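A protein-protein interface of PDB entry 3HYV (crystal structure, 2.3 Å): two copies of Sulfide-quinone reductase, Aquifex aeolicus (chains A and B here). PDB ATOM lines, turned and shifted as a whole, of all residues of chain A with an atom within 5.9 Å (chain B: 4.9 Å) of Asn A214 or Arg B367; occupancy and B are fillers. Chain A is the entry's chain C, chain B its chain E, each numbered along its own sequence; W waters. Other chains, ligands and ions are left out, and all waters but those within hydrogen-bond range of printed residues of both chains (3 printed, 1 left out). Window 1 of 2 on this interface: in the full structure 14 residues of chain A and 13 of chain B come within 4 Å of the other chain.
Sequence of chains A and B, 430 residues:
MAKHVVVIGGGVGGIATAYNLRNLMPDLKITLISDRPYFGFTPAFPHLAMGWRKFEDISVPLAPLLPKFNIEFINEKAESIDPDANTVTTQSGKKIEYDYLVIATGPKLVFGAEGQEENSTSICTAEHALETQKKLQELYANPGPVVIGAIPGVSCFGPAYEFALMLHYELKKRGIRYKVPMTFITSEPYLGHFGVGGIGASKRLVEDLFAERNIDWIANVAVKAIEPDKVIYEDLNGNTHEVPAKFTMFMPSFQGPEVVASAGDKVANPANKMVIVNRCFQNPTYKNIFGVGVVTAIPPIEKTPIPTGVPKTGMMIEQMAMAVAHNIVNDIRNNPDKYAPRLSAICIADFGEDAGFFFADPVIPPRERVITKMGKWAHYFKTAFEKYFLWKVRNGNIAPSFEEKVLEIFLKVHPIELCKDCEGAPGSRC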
ATOM      1  N   HIS A 168     -13.834  -3.932  24.948  1.00  0.00           N
ATOM      2  CA  HIS A 168     -12.590  -4.102  24.196  1.00  0.00           C
ATOM      3  C   HIS A 168     -11.756  -2.814  24.248  1.00  0.00           C
ATOM      4  O   HIS A 168     -10.566  -2.843  24.574  1.00  0.00           O
ATOM      5  CB  HIS A 168     -12.883  -4.503  22.747  1.00  0.00           C
ATOM      6  CG  HIS A 168     -11.696  -4.401  21.835  1.00  0.00           C
ATOM      7  ND1 HIS A 168     -10.698  -5.352  21.801  1.00  0.00           N
ATOM      8  CD2 HIS A 168     -11.347  -3.459  20.927  1.00  0.00           C
ATOM      9  CE1 HIS A 168      -9.785  -4.997  20.916  1.00  0.00           C
ATOM     10  NE2 HIS A 168     -10.156  -3.855  20.367  1.00  0.00           N
ATOM     11  N   ARG A 177      -5.852  -5.776  27.449  1.00  0.00           N
ATOM     12  CA  ARG A 177      -6.666  -6.598  26.534  1.00  0.00           C
ATOM     13  C   ARG A 177      -6.053  -7.979  26.216  1.00  0.00           C
ATOM     14  O   ARG A 177      -6.780  -8.968  26.070  1.00  0.00           O
ATOM     15  CB  ARG A 177      -7.006  -5.804  25.249  1.00  0.00           C
ATOM     16  CG  ARG A 177      -7.758  -6.568  24.143  1.00  0.00           C
ATOM     17  CD  ARG A 177      -9.191  -6.961  24.540  1.00  0.00           C
ATOM     18  NE  ARG A 177      -9.380  -8.401  24.383  1.00  0.00           N
ATOM     19  CZ  ARG A 177      -9.849  -9.004  23.294  1.00  0.00           C
ATOM     20  NH1 ARG A 177     -10.231  -8.309  22.235  1.00  0.00           N
ATOM     21  NH2 ARG A 177      -9.950 -10.324  23.278  1.00  0.00           N
ATOM     22  N   TYR A 178      -4.721  -8.041  26.146  1.00  0.00           N
ATOM     23  CA  TYR A 178      -3.994  -9.272  25.824  1.00  0.00           C
ATOM     24  C   TYR A 178      -4.042 -10.293  26.960  1.00  0.00           C
ATOM     25  O   TYR A 178      -3.583 -11.431  26.812  1.00  0.00           O
ATOM     26  CB  TYR A 178      -2.535  -8.960  25.406  1.00  0.00           C
ATOM     27  CG  TYR A 178      -1.592  -8.625  26.549  1.00  0.00           C
ATOM     28  CD1 TYR A 178      -0.594  -9.520  26.943  1.00  0.00           C
ATOM     29  CD2 TYR A 178      -1.699  -7.416  27.236  1.00  0.00           C
ATOM     30  CE1 TYR A 178       0.282  -9.211  27.997  1.00  0.00           C
ATOM     31  CE2 TYR A 178      -0.844  -7.101  28.285  1.00  0.00           C
ATOM     32  CZ  TYR A 178       0.144  -7.999  28.661  1.00  0.00           C
ATOM     33  OH  TYR A 178       0.983  -7.672  29.701  1.00  0.00           O
ATOM     34  N   MET A 182     -12.051 -12.784  24.881  1.00  0.00           N
ATOM     35  CA  MET A 182     -13.395 -12.253  24.622  1.00  0.00           C
ATOM     36  C   MET A 182     -14.148 -13.132  23.617  1.00  0.00           C
ATOM     37  O   MET A 182     -13.668 -13.363  22.511  1.00  0.00           O
ATOM     38  CB  MET A 182     -13.335 -10.786  24.131  1.00  0.00           C
ATOM     39  CG  MET A 182     -12.836  -9.775  25.185  1.00  0.00           C
ATOM     40  SD  MET A 182     -13.196  -8.018  24.877  1.00  0.00           S
ATOM     41  CE  MET A 182     -14.985  -7.988  25.122  1.00  0.00           C
ATOM     42  N   LEU A 209     -15.400  -6.635  11.498  1.00  0.00           N
ATOM     43  CA  LEU A 209     -15.084  -5.872  12.708  1.00  0.00           C
ATOM     44  C   LEU A 209     -14.603  -6.737  13.892  1.00  0.00           C
ATOM     45  O   LEU A 209     -13.593  -6.415  14.512  1.00  0.00           O
ATOM     46  CB  LEU A 209     -16.295  -5.031  13.114  1.00  0.00           C
ATOM     47  CG  LEU A 209     -16.193  -4.113  14.326  1.00  0.00           C
ATOM     48  CD1 LEU A 209     -15.212  -2.976  14.050  1.00  0.00           C
ATOM     49  CD2 LEU A 209     -17.564  -3.569  14.645  1.00  0.00           C
ATOM     50  N   PHE A 210     -15.329  -7.819  14.193  1.00  0.00           N
ATOM     51  CA  PHE A 210     -14.963  -8.775  15.254  1.00  0.00           C
ATOM     52  C   PHE A 210     -13.609  -9.458  15.001  1.00  0.00           C
ATOM     53  O   PHE A 210     -12.852  -9.723  15.941  1.00  0.00           O
ATOM     54  CB  PHE A 210     -16.065  -9.839  15.422  1.00  0.00           C
ATOM     55  CG  PHE A 210     -17.181  -9.447  16.372  1.00  0.00           C
ATOM     56  CD1 PHE A 210     -17.493  -8.107  16.621  1.00  0.00           C
ATOM     57  CD2 PHE A 210     -17.940 -10.428  17.001  1.00  0.00           C
ATOM     58  CE1 PHE A 210     -18.519  -7.763  17.500  1.00  0.00           C
ATOM     59  CE2 PHE A 210     -18.973 -10.086  17.871  1.00  0.00           C
ATOM     60  CZ  PHE A 210     -19.264  -8.752  18.120  1.00  0.00           C
ATOM     61  N   ALA A 211     -13.321  -9.742  13.730  1.00  0.00           N
ATOM     62  CA  ALA A 211     -12.041 -10.319  13.310  1.00  0.00           C
ATOM     63  C   ALA A 211     -10.864  -9.367  13.549  1.00  0.00           C
ATOM     64  O   ALA A 211      -9.811  -9.777  14.059  1.00  0.00           O
ATOM     65  CB  ALA A 211     -12.101 -10.728  11.844  1.00  0.00           C
ATOM     66  N   GLU A 212     -11.058  -8.102  13.179  1.00  0.00           N
ATOM     67  CA  GLU A 212     -10.055  -7.051  13.357  1.00  0.00           C
ATOM     68  C   GLU A 212      -9.767  -6.712  14.819  1.00  0.00           C
ATOM     69  O   GLU A 212      -8.672  -6.249  15.141  1.00  0.00           O
ATOM     70  CB  GLU A 212     -10.497  -5.776  12.616  1.00  0.00           C
ATOM     71  CG  GLU A 212     -10.660  -6.004  11.112  1.00  0.00           C
ATOM     72  CD  GLU A 212     -10.684  -4.725  10.287  1.00  0.00           C
ATOM     73  OE1 GLU A 212     -11.484  -3.807  10.605  1.00  0.00           O
ATOM     74  OE2 GLU A 212      -9.916  -4.663   9.300  1.00  0.00           O
ATOM     75  N   ARG A 213     -10.758  -6.921  15.690  1.00  0.00           N
ATOM     76  CA  ARG A 213     -10.642  -6.560  17.105  1.00  0.00           C
ATOM     77  C   ARG A 213     -10.534  -7.793  18.027  1.00  0.00           C
ATOM     78  O   ARG A 213     -10.624  -7.675  19.251  1.00  0.00           O
ATOM     79  CB  ARG A 213     -11.754  -5.562  17.507  1.00  0.00           C
ATOM     80  CG  ARG A 213     -11.611  -4.217  16.746  1.00  0.00           C
ATOM     81  CD  ARG A 213     -12.663  -3.124  17.036  1.00  0.00           C
ATOM     82  NE  ARG A 213     -12.515  -2.042  16.050  1.00  0.00           N
ATOM     83  CZ  ARG A 213     -13.113  -0.844  16.086  1.00  0.00           C
ATOM     84  NH1 ARG A 213     -13.926  -0.495  17.079  1.00  0.00           N
ATOM     85  NH2 ARG A 213     -12.882   0.028  15.110  1.00  0.00           N
ATOM     86  N   ASN A 214     -10.291  -8.955  17.410  1.00  0.00           N
ATOM     87  CA  ASN A 214     -10.124 -10.261  18.086  1.00  0.00           C
ATOM     88  C   ASN A 214     -11.249 -10.663  19.044  1.00  0.00           C
ATOM     89  O   ASN A 214     -10.999 -11.117  20.165  1.00  0.00           O
ATOM     90  CB  ASN A 214      -8.738 -10.402  18.765  1.00  0.00           C
ATOM     91  CG  ASN A 214      -8.378 -11.865  19.092  1.00  0.00           C
ATOM     92  OD1 ASN A 214      -8.405 -12.744  18.227  1.00  0.00           O
ATOM     93  ND2 ASN A 214      -8.033 -12.120  20.349  1.00  0.00           N
ATOM     94  N   ILE A 215     -12.490 -10.505  18.599  1.00  0.00           N
ATOM     95  CA  ILE A 215     -13.615 -11.048  19.359  1.00  0.00           C
ATOM     96  C   ILE A 215     -14.090 -12.327  18.676  1.00  0.00           C
ATOM     97  O   ILE A 215     -14.575 -12.287  17.547  1.00  0.00           O
ATOM     98  CB  ILE A 215     -14.754 -10.015  19.552  1.00  0.00           C
ATOM     99  CG1 ILE A 215     -14.244  -8.819  20.369  1.00  0.00           C
ATOM    100  CG2 ILE A 215     -15.968 -10.659  20.238  1.00  0.00           C
ATOM    101  CD1 ILE A 215     -14.926  -7.500  20.058  1.00  0.00           C
ATOM    102  N   ASP A 216     -13.896 -13.457  19.358  1.00  0.00           N
ATOM    103  CA  ASP A 216     -14.361 -14.767  18.909  1.00  0.00           C
ATOM    104  C   ASP A 216     -15.873 -14.798  19.000  1.00  0.00           C
ATOM    105  O   ASP A 216     -16.451 -14.081  19.817  1.00  0.00           O
ATOM    106  CB  ASP A 216     -13.788 -15.876  19.803  1.00  0.00           C
ATOM    107  CG  ASP A 216     -12.272 -15.929  19.782  1.00  0.00           C
ATOM    108  OD1 ASP A 216     -11.688 -15.963  18.671  1.00  0.00           O
ATOM    109  OD2 ASP A 216     -11.656 -15.953  20.878  1.00  0.00           O
ATOM    110  N   VAL B 196      -2.831 -20.083  13.326  1.00  0.00           N
ATOM    111  CA  VAL B 196      -2.995 -19.053  14.364  1.00  0.00           C
ATOM    112  C   VAL B 196      -4.467 -18.658  14.588  1.00  0.00           C
ATOM    113  O   VAL B 196      -4.766 -17.745  15.360  1.00  0.00           O
ATOM    114  CB  VAL B 196      -2.128 -17.776  14.070  1.00  0.00           C
ATOM    115  CG1 VAL B 196      -0.643 -18.120  14.034  1.00  0.00           C
ATOM    116  CG2 VAL B 196      -2.540 -17.104  12.774  1.00  0.00           C
ATOM    117  N   GLY B 198      -6.332 -17.371  12.244  1.00  0.00           N
ATOM    118  CA  GLY B 198      -6.560 -16.180  11.439  1.00  0.00           C
ATOM    119  C   GLY B 198      -5.886 -14.945  12.010  1.00  0.00           C
ATOM    120  O   GLY B 198      -5.631 -14.865  13.215  1.00  0.00           O
ATOM    121  N   ILE B 199      -5.578 -13.995  11.132  1.00  0.00           N
ATOM    122  CA  ILE B 199      -5.059 -12.684  11.519  1.00  0.00           C
ATOM    123  C   ILE B 199      -5.969 -11.634  10.876  1.00  0.00           C
ATOM    124  O   ILE B 199      -5.922 -11.414   9.662  1.00  0.00           O
ATOM    125  CB  ILE B 199      -3.577 -12.493  11.089  1.00  0.00           C
ATOM    126  CG1 ILE B 199      -2.689 -13.541  11.763  1.00  0.00           C
ATOM    127  CG2 ILE B 199      -3.092 -11.078  11.412  1.00  0.00           C
ATOM    128  CD1 ILE B 199      -1.310 -13.704  11.130  1.00  0.00           C
ATOM    129  N   GLY B 200      -6.815 -11.014  11.692  1.00  0.00           N
ATOM    130  CA  GLY B 200      -7.850 -10.132  11.186  1.00  0.00           C
ATOM    131  C   GLY B 200      -8.720 -10.882  10.194  1.00  0.00           C
ATOM    132  O   GLY B 200      -9.088 -12.039  10.421  1.00  0.00           O
ATOM    133  N   ALA B 360       0.388  -9.093  14.008  1.00  0.00           N
ATOM    134  CA  ALA B 360      -0.398  -9.601  15.147  1.00  0.00           C
ATOM    135  C   ALA B 360       0.372  -9.465  16.470  1.00  0.00           C
ATOM    136  O   ALA B 360       1.482  -9.964  16.579  1.00  0.00           O
ATOM    137  CB  ALA B 360      -0.788 -11.053  14.909  1.00  0.00           C
ATOM    138  N   ASP B 361      -0.227  -8.800  17.461  1.00  0.00           N
ATOM    139  CA  ASP B 361       0.409  -8.549  18.762  1.00  0.00           C
ATOM    140  C   ASP B 361      -0.491  -8.894  19.968  1.00  0.00           C
ATOM    141  O   ASP B 361      -1.430  -8.143  20.277  1.00  0.00           O
ATOM    142  CB  ASP B 361       0.859  -7.077  18.846  1.00  0.00           C
ATOM    143  CG  ASP B 361       1.406  -6.686  20.232  1.00  0.00           C
ATOM    144  OD1 ASP B 361       1.978  -7.544  20.938  1.00  0.00           O
ATOM    145  OD2 ASP B 361       1.253  -5.505  20.620  1.00  0.00           O
ATOM    146  N   PRO B 362      -0.210 -10.026  20.661  1.00  0.00           N
ATOM    147  CA  PRO B 362       0.705 -11.128  20.337  1.00  0.00           C
ATOM    148  C   PRO B 362       0.123 -12.060  19.280  1.00  0.00           C
ATOM    149  O   PRO B 362      -1.068 -11.993  19.004  1.00  0.00           O
ATOM    150  CB  PRO B 362       0.846 -11.879  21.671  1.00  0.00           C
ATOM    151  CG  PRO B 362       0.276 -10.958  22.719  1.00  0.00           C
ATOM    152  CD  PRO B 362      -0.803 -10.213  21.994  1.00  0.00           C
ATOM    153  N   VAL B 363       0.963 -12.905  18.686  1.00  0.00           N
ATOM    154  CA  VAL B 363       0.508 -13.932  17.748  1.00  0.00           C
ATOM    155  C   VAL B 363      -0.482 -14.882  18.423  1.00  0.00           C
ATOM    156  O   VAL B 363      -1.538 -15.182  17.853  1.00  0.00           O
ATOM    157  CB  VAL B 363       1.684 -14.721  17.124  1.00  0.00           C
ATOM    158  CG1 VAL B 363       1.172 -15.785  16.163  1.00  0.00           C
ATOM    159  CG2 VAL B 363       2.602 -13.785  16.386  1.00  0.00           C
ATOM    160  N   ILE B 364      -0.140 -15.330  19.631  1.00  0.00           N
ATOM    161  CA  ILE B 364      -1.025 -16.157  20.453  1.00  0.00           C
ATOM    162  C   ILE B 364      -2.054 -15.270  21.174  1.00  0.00           C
ATOM    163  O   ILE B 364      -1.670 -14.434  21.997  1.00  0.00           O
ATOM    164  CB  ILE B 364      -0.241 -17.001  21.502  1.00  0.00           C
ATOM    165  CG1 ILE B 364       0.806 -17.895  20.811  1.00  0.00           C
ATOM    166  CG2 ILE B 364      -1.203 -17.820  22.364  1.00  0.00           C
ATOM    167  CD1 ILE B 364       1.850 -18.490  21.735  1.00  0.00           C
ATOM    168  N   PRO B 365      -3.358 -15.459  20.864  1.00  0.00           N
ATOM    169  CA  PRO B 365      -4.506 -14.719  21.410  1.00  0.00           C
ATOM    170  C   PRO B 365      -4.727 -14.893  22.922  1.00  0.00           C
ATOM    171  O   PRO B 365      -4.253 -15.871  23.501  1.00  0.00           O
ATOM    172  CB  PRO B 365      -5.699 -15.313  20.645  1.00  0.00           C
ATOM    173  CG  PRO B 365      -5.122 -15.962  19.448  1.00  0.00           C
ATOM    174  CD  PRO B 365      -3.791 -16.461  19.873  1.00  0.00           C
ATOM    175  N   PRO B 366      -5.467 -13.964  23.566  1.00  0.00           N
ATOM    176  CA  PRO B 366      -6.126 -12.768  23.016  1.00  0.00           C
ATOM    177  C   PRO B 366      -5.131 -11.698  22.564  1.00  0.00           C
ATOM    178  O   PRO B 366      -4.061 -11.537  23.173  1.00  0.00           O
ATOM    179  CB  PRO B 366      -6.959 -12.259  24.188  1.00  0.00           C
ATOM    180  CG  PRO B 366      -6.242 -12.756  25.399  1.00  0.00           C
ATOM    181  CD  PRO B 366      -5.694 -14.093  25.017  1.00  0.00           C
ATOM    182  N   ARG B 367      -5.489 -10.978  21.505  1.00  0.00           N
ATOM    183  CA  ARG B 367      -4.596  -9.995  20.900  1.00  0.00           C
ATOM    184  C   ARG B 367      -4.931  -8.565  21.303  1.00  0.00           C
ATOM    185  O   ARG B 367      -6.092  -8.218  21.505  1.00  0.00           O
ATOM    186  CB  ARG B 367      -4.586 -10.144  19.369  1.00  0.00           C
ATOM    187  CG  ARG B 367      -4.286 -11.567  18.891  1.00  0.00           C
ATOM    188  CD  ARG B 367      -3.950 -11.610  17.422  1.00  0.00           C
ATOM    189  NE  ARG B 367      -3.470 -12.926  17.003  1.00  0.00           N
ATOM    190  CZ  ARG B 367      -4.097 -13.730  16.148  1.00  0.00           C
ATOM    191  NH1 ARG B 367      -3.567 -14.901  15.844  1.00  0.00           N
ATOM    192  NH2 ARG B 367      -5.247 -13.373  15.592  1.00  0.00           N
ATOM    193  N   GLU B 368      -3.897  -7.740  21.424  1.00  0.00           N
ATOM    194  CA  GLU B 368      -4.060  -6.297  21.617  1.00  0.00           C
ATOM    195  C   GLU B 368      -4.422  -5.604  20.296  1.00  0.00           C
ATOM    196  O   GLU B 368      -5.236  -4.685  20.297  1.00  0.00           O
ATOM    197  CB  GLU B 368      -2.790  -5.685  22.232  1.00  0.00           C
ATOM    198  CG  GLU B 368      -3.001  -4.363  22.982  1.00  0.00           C
ATOM    199  CD  GLU B 368      -3.479  -4.531  24.428  1.00  0.00           C
ATOM    200  OE1 GLU B 368      -3.489  -5.668  24.955  1.00  0.00           O
ATOM    201  OE2 GLU B 368      -3.843  -3.505  25.050  1.00  0.00           O
ATOM    202  N   ARG B 369      -3.825  -6.042  19.180  1.00  0.00           N
ATOM    203  CA  ARG B 369      -4.175  -5.514  17.841  1.00  0.00           C
ATOM    204  C   ARG B 369      -3.589  -6.310  16.663  1.00  0.00           C
ATOM    205  O   ARG B 369      -2.625  -7.059  16.842  1.00  0.00           O
ATOM    206  CB  ARG B 369      -3.828  -4.007  17.717  1.00  0.00           C
ATOM    207  CG  ARG B 369      -2.418  -3.681  17.192  1.00  0.00           C
ATOM    208  CD  ARG B 369      -2.070  -2.218  17.429  1.00  0.00           C
ATOM    209  NE  ARG B 369      -1.413  -2.078  18.722  1.00  0.00           N
ATOM    210  CZ  ARG B 369      -1.858  -1.365  19.747  1.00  0.00           C
ATOM    211  NH1 ARG B 369      -2.979  -0.664  19.660  1.00  0.00           N
ATOM    212  NH2 ARG B 369      -1.158  -1.348  20.867  1.00  0.00           N
ATOM    213  N   VAL B 370      -4.193  -6.145  15.480  1.00  0.00           N
ATOM    214  CA  VAL B 370      -3.730  -6.749  14.209  1.00  0.00           C
ATOM    215  C   VAL B 370      -3.773  -5.728  13.053  1.00  0.00           C
ATOM    216  O   VAL B 370      -4.472  -4.722  13.144  1.00  0.00           O
ATOM    217  CB  VAL B 370      -4.541  -8.028  13.785  1.00  0.00           C
ATOM    218  CG1 VAL B 370      -4.473  -9.117  14.848  1.00  0.00           C
ATOM    219  CG2 VAL B 370      -6.001  -7.698  13.438  1.00  0.00           C
HETATM  220  O   HOH W   1      -6.884  -4.438  16.098  1.00  0.00           O
HETATM  221  O   HOH W   2      -7.540 -11.750  14.665  1.00  0.00           O
HETATM  222  O   HOH W   3      -7.783  -4.132  18.581  1.00  0.00           O
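Water W1 lies within hydrogen-bond range of the backbone carbonyl oxygen of Glu A212 (2.7 Å) and the backbone NH of Val B370 (3.2 Å).
Water W2 lies within hydrogen-bond range of NH2 of Arg B367 (3.0 Å), O of Ala A211 (3.1 Å) and N of Gly B200 (3.1 Å).
Water W3 bridges a ring nitrogen (NE2) of His A168 (3.0 Å) and the backbone carbonyl oxygen (O) of Glu B368 (3.1 Å).
Among the printed residues, pairs that only touch across the chains: Arg A177 with Pro B366, Arg A177 with Arg B367, Tyr A178 with Pro B366, Ala A211 with Gly B200, Glu A212 with Val B370, Asn A214 with Pro B365 and Asn A214 with Pro B366.
No position is printed for both chains.
N of Arg A177 sits at hydrogen-bond distance from OE1 of Glu B368, 3.4 Å away.
The side-chain carboxylate (OE1) of Glu B368 sits at hydrogen-bond distance from the backbone NH (N) of Tyr A178 (2.9 Å).
N of Arg B367 sits close to ND2 of Asn A214, 3.0 Å away.
Printed residues of chain B within 4 Å of Arg A177: Pro B366 (3.7 Å), Arg B367 (3.5 Å) and Glu B368 (3.4 Å).
Met A182 touches none of the printed residues of chain B.
Of the printed residues of chain B, Glu A212 touches Val B370 (3.5 Å).
Asn A214 touches just these residues of chain B: Pro B365, Pro B366 and Arg B367.
Val B196 touches none of the printed residues of chain A.
Arg B367 touches just these residues of chain A: Arg A177 and Asn A214.
Of the printed residues of chain A, Val B370 touches Glu A212 (3.5 Å).
The nearest residue of chain A that does not touch Arg B367 is Tyr A178 (4.7 Å).
The nearest printed residue of chain B that does not touch Glu A212 is Gly B200 (4.3 Å).
A ring nitrogen (ND1) of His A168 is in hydrogen-bond range of the guanidinium group (NH1) of Arg A177.
The backbone carbonyl oxygen (O) of Val B196 lies within hydrogen-bond range of the guanidinium group (NH1) of Arg B367 (3.1 Å).
NH2 of Arg B367 lies within hydrogen-bond range of O of Gly B198 (2.8 Å).
O of Asp B361 sits at hydrogen-bond distance from N of Glu B368 (2.8 Å).
NE of Arg B367 sits close to O of Pro B362, at 3.3 Å.
The backbone carbonyl oxygen (O) of Val B363 is in hydrogen-bond range of the guanidinium group (NH1) of Arg B367, 2.9 Å away.
Printed residues of chain A that touch a printed residue of chain B: Arg A177, Tyr A178, Ala A211, Glu A212 and Asn A214.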
